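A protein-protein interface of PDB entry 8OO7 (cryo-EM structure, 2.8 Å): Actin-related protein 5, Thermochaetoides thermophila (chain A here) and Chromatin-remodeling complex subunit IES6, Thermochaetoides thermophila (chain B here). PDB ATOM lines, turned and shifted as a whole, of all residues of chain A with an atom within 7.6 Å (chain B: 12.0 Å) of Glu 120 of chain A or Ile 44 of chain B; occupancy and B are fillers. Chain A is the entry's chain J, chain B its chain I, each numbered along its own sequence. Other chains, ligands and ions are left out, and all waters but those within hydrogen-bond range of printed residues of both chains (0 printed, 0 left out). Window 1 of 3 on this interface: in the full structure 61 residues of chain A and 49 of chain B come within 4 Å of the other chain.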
ATOM      1  N   SER A  65     -26.096 -28.893  28.992  1.00  0.00           N
ATOM      2  CA  SER A  65     -26.545 -28.600  27.634  1.00  0.00           C
ATOM      3  C   SER A  65     -26.754 -29.863  26.812  1.00  0.00           C
ATOM      4  O   SER A  65     -27.536 -29.856  25.856  1.00  0.00           O
ATOM      5  CB  SER A  65     -25.539 -27.688  26.933  1.00  0.00           C
ATOM      6  OG  SER A  65     -25.220 -26.566  27.733  1.00  0.00           O
ATOM      7  N   ASN A 117     -34.315 -26.060  21.468  1.00  0.00           N
ATOM      8  CA  ASN A 117     -33.389 -26.345  22.558  1.00  0.00           C
ATOM      9  C   ASN A 117     -33.210 -25.106  23.425  1.00  0.00           C
ATOM     10  O   ASN A 117     -33.207 -23.978  22.923  1.00  0.00           O
ATOM     11  CB  ASN A 117     -32.031 -26.811  22.009  1.00  0.00           C
ATOM     12  CG  ASN A 117     -31.095 -27.310  23.093  1.00  0.00           C
ATOM     13  OD1 ASN A 117     -30.702 -26.564  23.989  1.00  0.00           O
ATOM     14  ND2 ASN A 117     -30.727 -28.583  23.010  1.00  0.00           N
ATOM     15  N   ALA A 118     -33.071 -25.331  24.736  1.00  0.00           N
ATOM     16  CA  ALA A 118     -32.948 -24.228  25.683  1.00  0.00           C
ATOM     17  C   ALA A 118     -31.656 -23.441  25.506  1.00  0.00           C
ATOM     18  O   ALA A 118     -31.633 -22.231  25.756  1.00  0.00           O
ATOM     19  CB  ALA A 118     -33.050 -24.761  27.109  1.00  0.00           C
ATOM     20  N   PHE A 119     -30.581 -24.096  25.083  1.00  0.00           N
ATOM     21  CA  PHE A 119     -29.263 -23.481  25.025  1.00  0.00           C
ATOM     22  C   PHE A 119     -28.966 -22.944  23.630  1.00  0.00           C
ATOM     23  O   PHE A 119     -29.384 -23.517  22.621  1.00  0.00           O
ATOM     24  CB  PHE A 119     -28.178 -24.478  25.433  1.00  0.00           C
ATOM     25  CG  PHE A 119     -28.284 -24.950  26.855  1.00  0.00           C
ATOM     26  CD1 PHE A 119     -29.117 -26.002  27.193  1.00  0.00           C
ATOM     27  CD2 PHE A 119     -27.529 -24.354  27.851  1.00  0.00           C
ATOM     28  CE1 PHE A 119     -29.208 -26.440  28.499  1.00  0.00           C
ATOM     29  CE2 PHE A 119     -27.610 -24.792  29.157  1.00  0.00           C
ATOM     30  CZ  PHE A 119     -28.452 -25.835  29.481  1.00  0.00           C
ATOM     31  N   GLU A 120     -28.228 -21.837  23.585  1.00  0.00           N
ATOM     32  CA  GLU A 120     -27.646 -21.364  22.335  1.00  0.00           C
ATOM     33  C   GLU A 120     -26.575 -22.343  21.871  1.00  0.00           C
ATOM     34  O   GLU A 120     -25.632 -22.636  22.613  1.00  0.00           O
ATOM     35  CB  GLU A 120     -27.064 -19.965  22.511  1.00  0.00           C
ATOM     36  CG  GLU A 120     -26.286 -19.473  21.306  1.00  0.00           C
ATOM     37  CD  GLU A 120     -26.072 -17.977  21.328  1.00  0.00           C
ATOM     38  OE1 GLU A 120     -26.911 -17.268  21.922  1.00  0.00           O
ATOM     39  OE2 GLU A 120     -25.072 -17.510  20.746  1.00  0.00           O
ATOM     40  N   ALA A 121     -26.728 -22.851  20.650  1.00  0.00           N
ATOM     41  CA  ALA A 121     -25.949 -23.997  20.199  1.00  0.00           C
ATOM     42  C   ALA A 121     -24.457 -23.697  20.222  1.00  0.00           C
ATOM     43  O   ALA A 121     -24.007 -22.666  19.715  1.00  0.00           O
ATOM     44  CB  ALA A 121     -26.384 -24.401  18.792  1.00  0.00           C
ATOM     45  N   GLY A 122     -23.693 -24.614  20.810  1.00  0.00           N
ATOM     46  CA  GLY A 122     -22.277 -24.413  21.033  1.00  0.00           C
ATOM     47  C   GLY A 122     -21.917 -23.477  22.159  1.00  0.00           C
ATOM     48  O   GLY A 122     -20.810 -22.931  22.162  1.00  0.00           O
ATOM     49  N   THR A 123     -22.818 -23.267  23.116  1.00  0.00           N
ATOM     50  CA  THR A 123     -22.536 -22.472  24.303  1.00  0.00           C
ATOM     51  C   THR A 123     -23.147 -23.162  25.512  1.00  0.00           C
ATOM     52  O   THR A 123     -23.993 -24.049  25.385  1.00  0.00           O
ATOM     53  CB  THR A 123     -23.081 -21.035  24.200  1.00  0.00           C
ATOM     54  OG1 THR A 123     -24.494 -21.037  24.436  1.00  0.00           O
ATOM     55  CG2 THR A 123     -22.794 -20.417  22.837  1.00  0.00           C
ATOM     56  N   GLY A 124     -22.685 -22.764  26.693  1.00  0.00           N
ATOM     57  CA  GLY A 124     -23.170 -23.317  27.937  1.00  0.00           C
ATOM     58  C   GLY A 124     -24.293 -22.528  28.565  1.00  0.00           C
ATOM     59  O   GLY A 124     -24.719 -22.846  29.680  1.00  0.00           O
ATOM     60  N   ILE A 125     -24.796 -21.516  27.869  1.00  0.00           N
ATOM     61  CA  ILE A 125     -25.711 -20.533  28.433  1.00  0.00           C
ATOM     62  C   ILE A 125     -27.117 -20.820  27.924  1.00  0.00           C
ATOM     63  O   ILE A 125     -27.318 -21.059  26.727  1.00  0.00           O
ATOM     64  CB  ILE A 125     -25.253 -19.107  28.090  1.00  0.00           C
ATOM     65  CG1 ILE A 125     -24.052 -18.746  28.967  1.00  0.00           C
ATOM     66  CG2 ILE A 125     -26.378 -18.118  28.285  1.00  0.00           C
ATOM     67  CD1 ILE A 125     -23.189 -17.635  28.433  1.00  0.00           C
ATOM     68  N   VAL A 126     -28.087 -20.811  28.841  1.00  0.00           N
ATOM     69  CA  VAL A 126     -29.494 -20.903  28.471  1.00  0.00           C
ATOM     70  C   VAL A 126     -29.942 -19.614  27.797  1.00  0.00           C
ATOM     71  O   VAL A 126     -29.608 -18.507  28.240  1.00  0.00           O
ATOM     72  CB  VAL A 126     -30.352 -21.211  29.709  1.00  0.00           C
ATOM     73  CG1 VAL A 126     -31.814 -21.254  29.336  1.00  0.00           C
ATOM     74  CG2 VAL A 126     -29.933 -22.521  30.326  1.00  0.00           C
ATOM     75  N   SER A 127     -30.700 -19.753  26.712  1.00  0.00           N
ATOM     76  CA  SER A 127     -31.135 -18.608  25.918  1.00  0.00           C
ATOM     77  C   SER A 127     -32.587 -18.673  25.460  1.00  0.00           C
ATOM     78  O   SER A 127     -33.181 -17.614  25.236  1.00  0.00           O
ATOM     79  CB  SER A 127     -30.234 -18.435  24.691  1.00  0.00           C
ATOM     80  OG  SER A 127     -30.744 -17.435  23.829  1.00  0.00           O
ATOM     81  N   ASN A 128     -33.181 -19.854  25.297  1.00  0.00           N
ATOM     82  CA  ASN A 128     -34.610 -19.987  25.013  1.00  0.00           C
ATOM     83  C   ASN A 128     -35.321 -20.357  26.311  1.00  0.00           C
ATOM     84  O   ASN A 128     -35.439 -21.528  26.673  1.00  0.00           O
ATOM     85  CB  ASN A 128     -34.847 -21.018  23.917  1.00  0.00           C
ATOM     86  CG  ASN A 128     -34.143 -20.661  22.623  1.00  0.00           C
ATOM     87  OD1 ASN A 128     -34.319 -19.565  22.090  1.00  0.00           O
ATOM     88  ND2 ASN A 128     -33.325 -21.578  22.121  1.00  0.00           N
ATOM     89  N   ASN A 164     -21.115 -17.473  33.986  1.00  0.00           N
ATOM     90  CA  ASN A 164     -22.460 -17.338  33.436  1.00  0.00           C
ATOM     91  C   ASN A 164     -22.916 -15.885  33.412  1.00  0.00           C
ATOM     92  O   ASN A 164     -22.616 -15.109  34.323  1.00  0.00           O
ATOM     93  CB  ASN A 164     -23.444 -18.179  34.250  1.00  0.00           C
ATOM     94  CG  ASN A 164     -24.849 -18.130  33.691  1.00  0.00           C
ATOM     95  OD1 ASN A 164     -25.042 -18.077  32.478  1.00  0.00           O
ATOM     96  ND2 ASN A 164     -25.840 -18.150  34.574  1.00  0.00           N
ATOM     97  N   LEU A 165     -23.641 -15.528  32.359  1.00  0.00           N
ATOM     98  CA  LEU A 165     -24.026 -14.140  32.159  1.00  0.00           C
ATOM     99  C   LEU A 165     -25.068 -13.720  33.194  1.00  0.00           C
ATOM    100  O   LEU A 165     -25.969 -14.499  33.518  1.00  0.00           O
ATOM    101  CB  LEU A 165     -24.577 -13.928  30.751  1.00  0.00           C
ATOM    102  CG  LEU A 165     -23.608 -14.221  29.608  1.00  0.00           C
ATOM    103  CD1 LEU A 165     -24.311 -14.079  28.274  1.00  0.00           C
ATOM    104  CD2 LEU A 165     -22.404 -13.302  29.678  1.00  0.00           C
ATOM    105  N   SER A 168     -28.697 -14.120  32.123  1.00  0.00           N
ATOM    106  CA  SER A 168     -29.136 -15.512  32.116  1.00  0.00           C
ATOM    107  C   SER A 168     -29.471 -16.000  33.519  1.00  0.00           C
ATOM    108  O   SER A 168     -30.453 -16.725  33.713  1.00  0.00           O
ATOM    109  CB  SER A 168     -28.059 -16.393  31.489  1.00  0.00           C
ATOM    110  OG  SER A 168     -27.746 -15.946  30.185  1.00  0.00           O
ATOM    111  N   TYR A 210     -20.165 -30.736  26.746  1.00  0.00           N
ATOM    112  CA  TYR A 210     -20.837 -30.439  25.487  1.00  0.00           C
ATOM    113  C   TYR A 210     -20.516 -29.024  25.019  1.00  0.00           C
ATOM    114  O   TYR A 210     -20.216 -28.799  23.841  1.00  0.00           O
ATOM    115  CB  TYR A 210     -22.343 -30.627  25.673  1.00  0.00           C
ATOM    116  CG  TYR A 210     -23.134 -30.875  24.411  1.00  0.00           C
ATOM    117  CD1 TYR A 210     -23.020 -32.067  23.713  1.00  0.00           C
ATOM    118  CD2 TYR A 210     -24.017 -29.919  23.934  1.00  0.00           C
ATOM    119  CE1 TYR A 210     -23.741 -32.285  22.556  1.00  0.00           C
ATOM    120  CE2 TYR A 210     -24.747 -30.133  22.790  1.00  0.00           C
ATOM    121  CZ  TYR A 210     -24.604 -31.313  22.103  1.00  0.00           C
ATOM    122  OH  TYR A 210     -25.351 -31.527  20.968  1.00  0.00           O
ATOM    123  N   SER A 211     -20.585 -28.052  25.928  1.00  0.00           N
ATOM    124  CA  SER A 211     -20.543 -26.657  25.504  1.00  0.00           C
ATOM    125  C   SER A 211     -19.133 -26.181  25.181  1.00  0.00           C
ATOM    126  O   SER A 211     -18.942 -25.378  24.260  1.00  0.00           O
ATOM    127  CB  SER A 211     -21.155 -25.769  26.584  1.00  0.00           C
ATOM    128  OG  SER A 211     -20.541 -25.981  27.847  1.00  0.00           O
ATOM    129  N   TRP A 236     -20.192 -30.950  21.545  1.00  0.00           N
ATOM    130  CA  TRP A 236     -21.072 -30.463  20.486  1.00  0.00           C
ATOM    131  C   TRP A 236     -20.280 -30.159  19.224  1.00  0.00           C
ATOM    132  O   TRP A 236     -20.624 -30.618  18.130  1.00  0.00           O
ATOM    133  CB  TRP A 236     -21.802 -29.204  20.948  1.00  0.00           C
ATOM    134  CG  TRP A 236     -22.749 -28.657  19.924  1.00  0.00           C
ATOM    135  CD1 TRP A 236     -23.991 -29.127  19.631  1.00  0.00           C
ATOM    136  CD2 TRP A 236     -22.502 -27.584  19.008  1.00  0.00           C
ATOM    137  NE1 TRP A 236     -24.553 -28.389  18.621  1.00  0.00           N
ATOM    138  CE2 TRP A 236     -23.656 -27.438  18.217  1.00  0.00           C
ATOM    139  CE3 TRP A 236     -21.420 -26.727  18.788  1.00  0.00           C
ATOM    140  CZ2 TRP A 236     -23.762 -26.467  17.227  1.00  0.00           C
ATOM    141  CZ3 TRP A 236     -21.529 -25.762  17.809  1.00  0.00           C
ATOM    142  CH2 TRP A 236     -22.691 -25.641  17.038  1.00  0.00           C
ATOM    143  N   ARG B  39     -40.052 -10.505  25.034  1.00  0.00           N
ATOM    144  CA  ARG B  39     -38.726 -10.257  24.476  1.00  0.00           C
ATOM    145  C   ARG B  39     -37.593 -10.936  25.239  1.00  0.00           C
ATOM    146  O   ARG B  39     -36.425 -10.706  24.907  1.00  0.00           O
ATOM    147  CB  ARG B  39     -38.460  -8.749  24.408  1.00  0.00           C
ATOM    148  CG  ARG B  39     -39.368  -8.006  23.442  1.00  0.00           C
ATOM    149  CD  ARG B  39     -39.075  -6.515  23.434  1.00  0.00           C
ATOM    150  NE  ARG B  39     -37.710  -6.226  23.011  1.00  0.00           N
ATOM    151  CZ  ARG B  39     -37.320  -6.145  21.745  1.00  0.00           C
ATOM    152  NH1 ARG B  39     -38.164  -6.354  20.748  1.00  0.00           N
ATOM    153  NH2 ARG B  39     -36.052  -5.853  21.475  1.00  0.00           N
ATOM    154  N   ARG B  40     -37.901 -11.752  26.248  1.00  0.00           N
ATOM    155  CA  ARG B  40     -36.870 -12.247  27.156  1.00  0.00           C
ATOM    156  C   ARG B  40     -35.845 -13.150  26.471  1.00  0.00           C
ATOM    157  O   ARG B  40     -34.695 -13.219  26.919  1.00  0.00           O
ATOM    158  CB  ARG B  40     -37.528 -12.969  28.334  1.00  0.00           C
ATOM    159  CG  ARG B  40     -38.187 -14.295  27.995  1.00  0.00           C
ATOM    160  CD  ARG B  40     -38.698 -14.980  29.250  1.00  0.00           C
ATOM    161  NE  ARG B  40     -39.503 -16.158  28.949  1.00  0.00           N
ATOM    162  CZ  ARG B  40     -39.850 -17.075  29.841  1.00  0.00           C
ATOM    163  NH1 ARG B  40     -39.430 -17.014  31.094  1.00  0.00           N
ATOM    164  NH2 ARG B  40     -40.634 -18.082  29.464  1.00  0.00           N
ATOM    165  N   ASN B  41     -36.221 -13.843  25.400  1.00  0.00           N
ATOM    166  CA  ASN B  41     -35.264 -14.680  24.670  1.00  0.00           C
ATOM    167  C   ASN B  41     -34.285 -13.811  23.886  1.00  0.00           C
ATOM    168  O   ASN B  41     -34.618 -13.273  22.828  1.00  0.00           O
ATOM    169  CB  ASN B  41     -36.003 -15.646  23.753  1.00  0.00           C
ATOM    170  CG  ASN B  41     -36.645 -16.790  24.512  1.00  0.00           C
ATOM    171  OD1 ASN B  41     -36.732 -16.763  25.740  1.00  0.00           O
ATOM    172  ND2 ASN B  41     -37.092 -17.808  23.784  1.00  0.00           N
ATOM    173  N   LYS B  42     -33.060 -13.685  24.398  1.00  0.00           N
ATOM    174  CA  LYS B  42     -32.009 -12.891  23.772  1.00  0.00           C
ATOM    175  C   LYS B  42     -30.758 -13.740  23.583  1.00  0.00           C
ATOM    176  O   LYS B  42     -30.463 -14.616  24.401  1.00  0.00           O
ATOM    177  CB  LYS B  42     -31.691 -11.627  24.580  1.00  0.00           C
ATOM    178  CG  LYS B  42     -32.870 -10.669  24.679  1.00  0.00           C
ATOM    179  CD  LYS B  42     -32.462  -9.317  25.236  1.00  0.00           C
ATOM    180  CE  LYS B  42     -32.020  -9.410  26.676  1.00  0.00           C
ATOM    181  NZ  LYS B  42     -31.887  -8.063  27.289  1.00  0.00           N
ATOM    182  N   THR B  43     -30.036 -13.485  22.491  1.00  0.00           N
ATOM    183  CA  THR B  43     -28.797 -14.184  22.180  1.00  0.00           C
ATOM    184  C   THR B  43     -27.616 -13.608  22.960  1.00  0.00           C
ATOM    185  O   THR B  43     -27.664 -12.494  23.490  1.00  0.00           O
ATOM    186  CB  THR B  43     -28.499 -14.121  20.682  1.00  0.00           C
ATOM    187  OG1 THR B  43     -28.392 -12.752  20.272  1.00  0.00           O
ATOM    188  CG2 THR B  43     -29.603 -14.798  19.889  1.00  0.00           C
ATOM    189  N   ILE B  44     -26.542 -14.404  23.013  1.00  0.00           N
ATOM    190  CA  ILE B  44     -25.298 -14.010  23.680  1.00  0.00           C
ATOM    191  C   ILE B  44     -24.838 -12.632  23.222  1.00  0.00           C
ATOM    192  O   ILE B  44     -24.476 -11.776  24.036  1.00  0.00           O
ATOM    193  CB  ILE B  44     -24.208 -15.066  23.427  1.00  0.00           C
ATOM    194  CG1 ILE B  44     -24.612 -16.412  24.021  1.00  0.00           C
ATOM    195  CG2 ILE B  44     -22.880 -14.612  24.007  1.00  0.00           C
ATOM    196  CD1 ILE B  44     -24.722 -16.396  25.507  1.00  0.00           C
ATOM    197  N   LYS B  45     -24.832 -12.402  21.907  1.00  0.00           N
ATOM    198  CA  LYS B  45     -24.399 -11.110  21.383  1.00  0.00           C
ATOM    199  C   LYS B  45     -25.308  -9.982  21.858  1.00  0.00           C
ATOM    200  O   LYS B  45     -24.830  -8.900  22.219  1.00  0.00           O
ATOM    201  CB  LYS B  45     -24.339 -11.148  19.856  1.00  0.00           C
ATOM    202  CG  LYS B  45     -23.810  -9.867  19.226  1.00  0.00           C
ATOM    203  CD  LYS B  45     -23.718  -9.985  17.713  1.00  0.00           C
ATOM    204  CE  LYS B  45     -23.237  -8.685  17.083  1.00  0.00           C
ATOM    205  NZ  LYS B  45     -23.155  -8.779  15.598  1.00  0.00           N
ATOM    206  N   ALA B  46     -26.621 -10.216  21.862  1.00  0.00           N
ATOM    207  CA  ALA B  46     -27.555  -9.220  22.380  1.00  0.00           C
ATOM    208  C   ALA B  46     -27.330  -8.959  23.867  1.00  0.00           C
ATOM    209  O   ALA B  46     -27.296  -7.805  24.305  1.00  0.00           O
ATOM    210  CB  ALA B  46     -28.992  -9.671  22.119  1.00  0.00           C
ATOM    211  N   ILE B  47     -27.182 -10.024  24.658  1.00  0.00           N
ATOM    212  CA  ILE B  47     -26.941  -9.868  26.092  1.00  0.00           C
ATOM    213  C   ILE B  47     -25.645  -9.106  26.346  1.00  0.00           C
ATOM    214  O   ILE B  47     -25.616  -8.134  27.111  1.00  0.00           O
ATOM    215  CB  ILE B  47     -26.928 -11.242  26.784  1.00  0.00           C
ATOM    216  CG1 ILE B  47     -28.297 -11.910  26.665  1.00  0.00           C
ATOM    217  CG2 ILE B  47     -26.531 -11.099  28.241  1.00  0.00           C
ATOM    218  CD1 ILE B  47     -28.276 -13.401  26.904  1.00  0.00           C
ATOM    219  N   LEU B  48     -24.553  -9.533  25.709  1.00  0.00           N
ATOM    220  CA  LEU B  48     -23.279  -8.846  25.889  1.00  0.00           C
ATOM    221  C   LEU B  48     -23.336  -7.410  25.380  1.00  0.00           C
ATOM    222  O   LEU B  48     -22.824  -6.492  26.033  1.00  0.00           O
ATOM    223  CB  LEU B  48     -22.164  -9.617  25.187  1.00  0.00           C
ATOM    224  CG  LEU B  48     -21.792 -10.959  25.817  1.00  0.00           C
ATOM    225  CD1 LEU B  48     -20.782 -11.687  24.954  1.00  0.00           C
ATOM    226  CD2 LEU B  48     -21.257 -10.758  27.220  1.00  0.00           C
ATOM    227  N   GLY B  49     -23.944  -7.197  24.213  1.00  0.00           N
ATOM    228  CA  GLY B  49     -24.053  -5.848  23.678  1.00  0.00           C
ATOM    229  C   GLY B  49     -24.863  -4.916  24.559  1.00  0.00           C
ATOM    230  O   GLY B  49     -24.525  -3.740  24.710  1.00  0.00           O
ATOM    231  N   GLU B  50     -25.938  -5.428  25.160  1.00  0.00           N
ATOM    232  CA  GLU B  50     -26.724  -4.636  26.097  1.00  0.00           C
ATOM    233  C   GLU B  50     -26.043  -4.474  27.451  1.00  0.00           C
ATOM    234  O   GLU B  50     -26.246  -3.454  28.118  1.00  0.00           O
ATOM    235  CB  GLU B  50     -28.103  -5.267  26.282  1.00  0.00           C
ATOM    236  CG  GLU B  50     -29.005  -5.134  25.066  1.00  0.00           C
ATOM    237  CD  GLU B  50     -30.322  -5.864  25.235  1.00  0.00           C
ATOM    238  OE1 GLU B  50     -30.569  -6.398  26.336  1.00  0.00           O
ATOM    239  OE2 GLU B  50     -31.110  -5.902  24.267  1.00  0.00           O
ATOM    240  N   SER B  51     -25.238  -5.449  27.873  1.00  0.00           N
ATOM    241  CA  SER B  51     -24.507  -5.294  29.126  1.00  0.00           C
ATOM    242  C   SER B  51     -23.380  -4.276  29.002  1.00  0.00           C
ATOM    243  O   SER B  51     -23.035  -3.617  29.989  1.00  0.00           O
ATOM    244  CB  SER B  51     -23.952  -6.643  29.582  1.00  0.00           C
ATOM    245  OG  SER B  51     -24.988  -7.595  29.746  1.00  0.00           O
ATOM    246  N   GLN B  52     -22.796  -4.138  27.817  1.00  0.00           N
ATOM    247  CA  GLN B  52     -21.728  -3.168  27.594  1.00  0.00           C
ATOM    248  C   GLN B  52     -22.208  -1.741  27.838  1.00  0.00           C
ATOM    249  O   GLN B  52     -23.238  -1.325  27.310  1.00  0.00           O
ATOM    250  CB  GLN B  52     -21.172  -3.297  26.175  1.00  0.00           C
ATOM    251  CG  GLN B  52     -20.013  -2.363  25.874  1.00  0.00           C
ATOM    252  CD  GLN B  52     -19.396  -2.624  24.515  1.00  0.00           C
ATOM    253  OE1 GLN B  52     -19.889  -3.449  23.746  1.00  0.00           O
ATOM    254  NE2 GLN B  52     -18.310  -1.921  24.212  1.00  0.00           N
ATOM    255  N   THR B 155     -15.697 -13.372  33.122  1.00  0.00           N
ATOM    256  CA  THR B 155     -16.871 -12.651  32.647  1.00  0.00           C
ATOM    257  C   THR B 155     -17.003 -12.753  31.131  1.00  0.00           C
ATOM    258  O   THR B 155     -17.202 -11.744  30.453  1.00  0.00           O
ATOM    259  CB  THR B 155     -16.825 -11.164  33.048  1.00  0.00           C
ATOM    260  OG1 THR B 155     -15.755 -10.508  32.357  1.00  0.00           O
ATOM    261  CG2 THR B 155     -16.618 -11.021  34.547  1.00  0.00           C
ATOM    262  N   ASN B 156     -16.882 -13.976  30.610  1.00  0.00           N
ATOM    263  CA  ASN B 156     -16.735 -14.218  29.172  1.00  0.00           C
ATOM    264  C   ASN B 156     -15.559 -13.423  28.607  1.00  0.00           C
ATOM    265  O   ASN B 156     -15.605 -12.895  27.494  1.00  0.00           O
ATOM    266  CB  ASN B 156     -18.030 -13.908  28.422  1.00  0.00           C
ATOM    267  CG  ASN B 156     -19.051 -15.025  28.545  1.00  0.00           C
ATOM    268  OD1 ASN B 156     -19.207 -15.618  29.613  1.00  0.00           O
ATOM    269  ND2 ASN B 156     -19.734 -15.332  27.448  1.00  0.00           N
ATOM    270  N   ILE B 157     -14.498 -13.330  29.406  1.00  0.00           N
ATOM    271  CA  ILE B 157     -13.179 -12.854  29.000  1.00  0.00           C
ATOM    272  C   ILE B 157     -12.178 -13.963  29.296  1.00  0.00           C
ATOM    273  O   ILE B 157     -11.005 -13.707  29.589  1.00  0.00           O
ATOM    274  CB  ILE B 157     -12.812 -11.537  29.709  1.00  0.00           C
ATOM    275  CG1 ILE B 157     -12.747 -11.740  31.222  1.00  0.00           C
ATOM    276  CG2 ILE B 157     -13.824 -10.454  29.368  1.00  0.00           C
ATOM    277  CD1 ILE B 157     -12.287 -10.521  31.981  1.00  0.00           C
ATOM    278  N   GLU B 158     -12.648 -15.204  29.220  1.00  0.00           N
ATOM    279  CA  GLU B 158     -11.866 -16.397  29.516  1.00  0.00           C
ATOM    280  C   GLU B 158     -11.291 -17.084  28.282  1.00  0.00           C
ATOM    281  O   GLU B 158     -10.569 -18.074  28.429  1.00  0.00           O
ATOM    282  CB  GLU B 158     -12.737 -17.391  30.290  1.00  0.00           C
ATOM    283  CG  GLU B 158     -13.233 -16.868  31.625  1.00  0.00           C
ATOM    284  CD  GLU B 158     -13.805 -17.961  32.498  1.00  0.00           C
ATOM    285  OE1 GLU B 158     -14.188 -19.014  31.950  1.00  0.00           O
ATOM    286  OE2 GLU B 158     -13.894 -17.759  33.728  1.00  0.00           O
ATOM    287  N   SER B 159     -11.600 -16.613  27.076  1.00  0.00           N
ATOM    288  CA  SER B 159     -10.992 -17.186  25.880  1.00  0.00           C
ATOM    289  C   SER B 159      -9.536 -16.742  25.724  1.00  0.00           C
ATOM    290  O   SER B 159      -9.136 -15.668  26.183  1.00  0.00           O
ATOM    291  CB  SER B 159     -11.795 -16.796  24.638  1.00  0.00           C
ATOM    292  OG  SER B 159     -11.981 -15.393  24.572  1.00  0.00           O
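O of Lys 42 of chain B is in hydrogen-bond range of OG of Ser 127 of chain A, at 2.9 Å.
The backbone NH (N) of Ile 44 of chain B is in hydrogen-bond range of the side-chain carboxylate (OE1) of Glu 120 of chain A, 3.1 Å away.
The backbone NH (N) of Glu 120 of chain A sits at hydrogen-bond distance from the backbone carbonyl oxygen (O) of Ile 125 of chain A.
The backbone carbonyl oxygen (O) of Ile 47 of chain B lies within hydrogen-bond range of the side-chain hydroxyl (OG) of Ser 51 of chain B, 2.8 Å away.
The backbone NH (N) of Asn 128 of chain A is in hydrogen-bond range of the backbone carbonyl oxygen (O) of Ala 118 of chain A, 2.9 Å away.
NZ of Lys 42 of chain B lies within salt-bridge range of OE2 of Glu 50 of chain B (3.8 Å).
The backbone carbonyl oxygen (O) of Glu 120 of chain A lies within hydrogen-bond range of the side-chain hydroxyl (OG1) of Thr 123 of chain A, at 2.7 Å.
The side-chain hydroxyl of Thr 43 of chain B sits at hydrogen-bond distance from the backbone NH of Ala 46 of chain B (3.5 Å).
Among the printed residues, merely in contact across the chains: Glu 120 of chain A with Thr 43 of chain B (3.6 Å), Ile 125 of chain A with Ile 44 of chain B (3.5 Å), Ser 127 of chain A with Asn 41 of chain B (3.6 Å), Asn 128 of chain A with Asn 41 of chain B (3.5 Å), Leu 165 of chain A with Ile 44 of chain B (3.6 Å), Leu 165 of chain A with Ile 47 of chain B (3.7 Å), Leu 165 of chain A with Leu 48 of chain B (3.7 Å) and Leu 165 of chain A with Asn 156 of chain B (3.9 Å).
No residue of chain B comes within 4 Å of Asn 117 of chain A.
No residue of chain B comes within 4 Å of Ala 118 of chain A.
Of chain B, only Thr 43 and Ile 44 come within 4 Å of Glu 120 of chain A.
No residue of chain B comes within 4 Å of Ala 121 of chain A.
No residue of chain B comes within 4 Å of Gly 124 of chain A.
Ile 125 of chain A touches just one residue of chain B: Ile 44.
No residue of chain B comes within 4 Å of Val 126 of chain A.
Of chain B, only Asn 41 and Lys 42 come within 4 Å of Ser 127 of chain A.
Printed residues of chain B within 4 Å of Leu 165 of chain A: Ile 44, Ile 47, Leu 48 and Asn 156.
Arg 40 of chain B touches none of the printed residues of chain A.
Of the printed residues of chain A, Lys 42 of chain B touches Ser 127 (2.9 Å).
Printed residues of chain A within 4 Å of Thr 43 of chain B: Glu 120.
Of chain A, only Glu 120 (3.1 Å), Ile 125 (3.5 Å) and Leu 165 (3.6 Å) come within 4 Å of Ile 44 of chain B.
Ala 46 of chain B touches none of the printed residues of chain A.
Printed residues of chain A within 4 Å of Ile 47 of chain B: Leu 165.
Printed residues of chain A within 4 Å of Leu 48 of chain B: Leu 165 (3.7 Å).
The nearest residue of chain A that does not touch Ile 44 of chain B is Thr 123 of chain A (4.6 Å).
The nearest printed residue of chain B that does not touch Leu 165 of chain A is Thr 155 of chain B (5.5 Å).
Of the 19 printed residues of chain A, 5 touch a printed residue of chain B.
Hydrophobic or aromatic side chains of chain A within 4 Å of the printed part of chain B: Ile 125 and Leu 165.
Hydrophobic or aromatic side chains of chain B within 4 Å of the printed part of chain A: Ile 44, Ile 47 and Leu 48.
Among the printed residues, 10 pairs touch across the chains.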
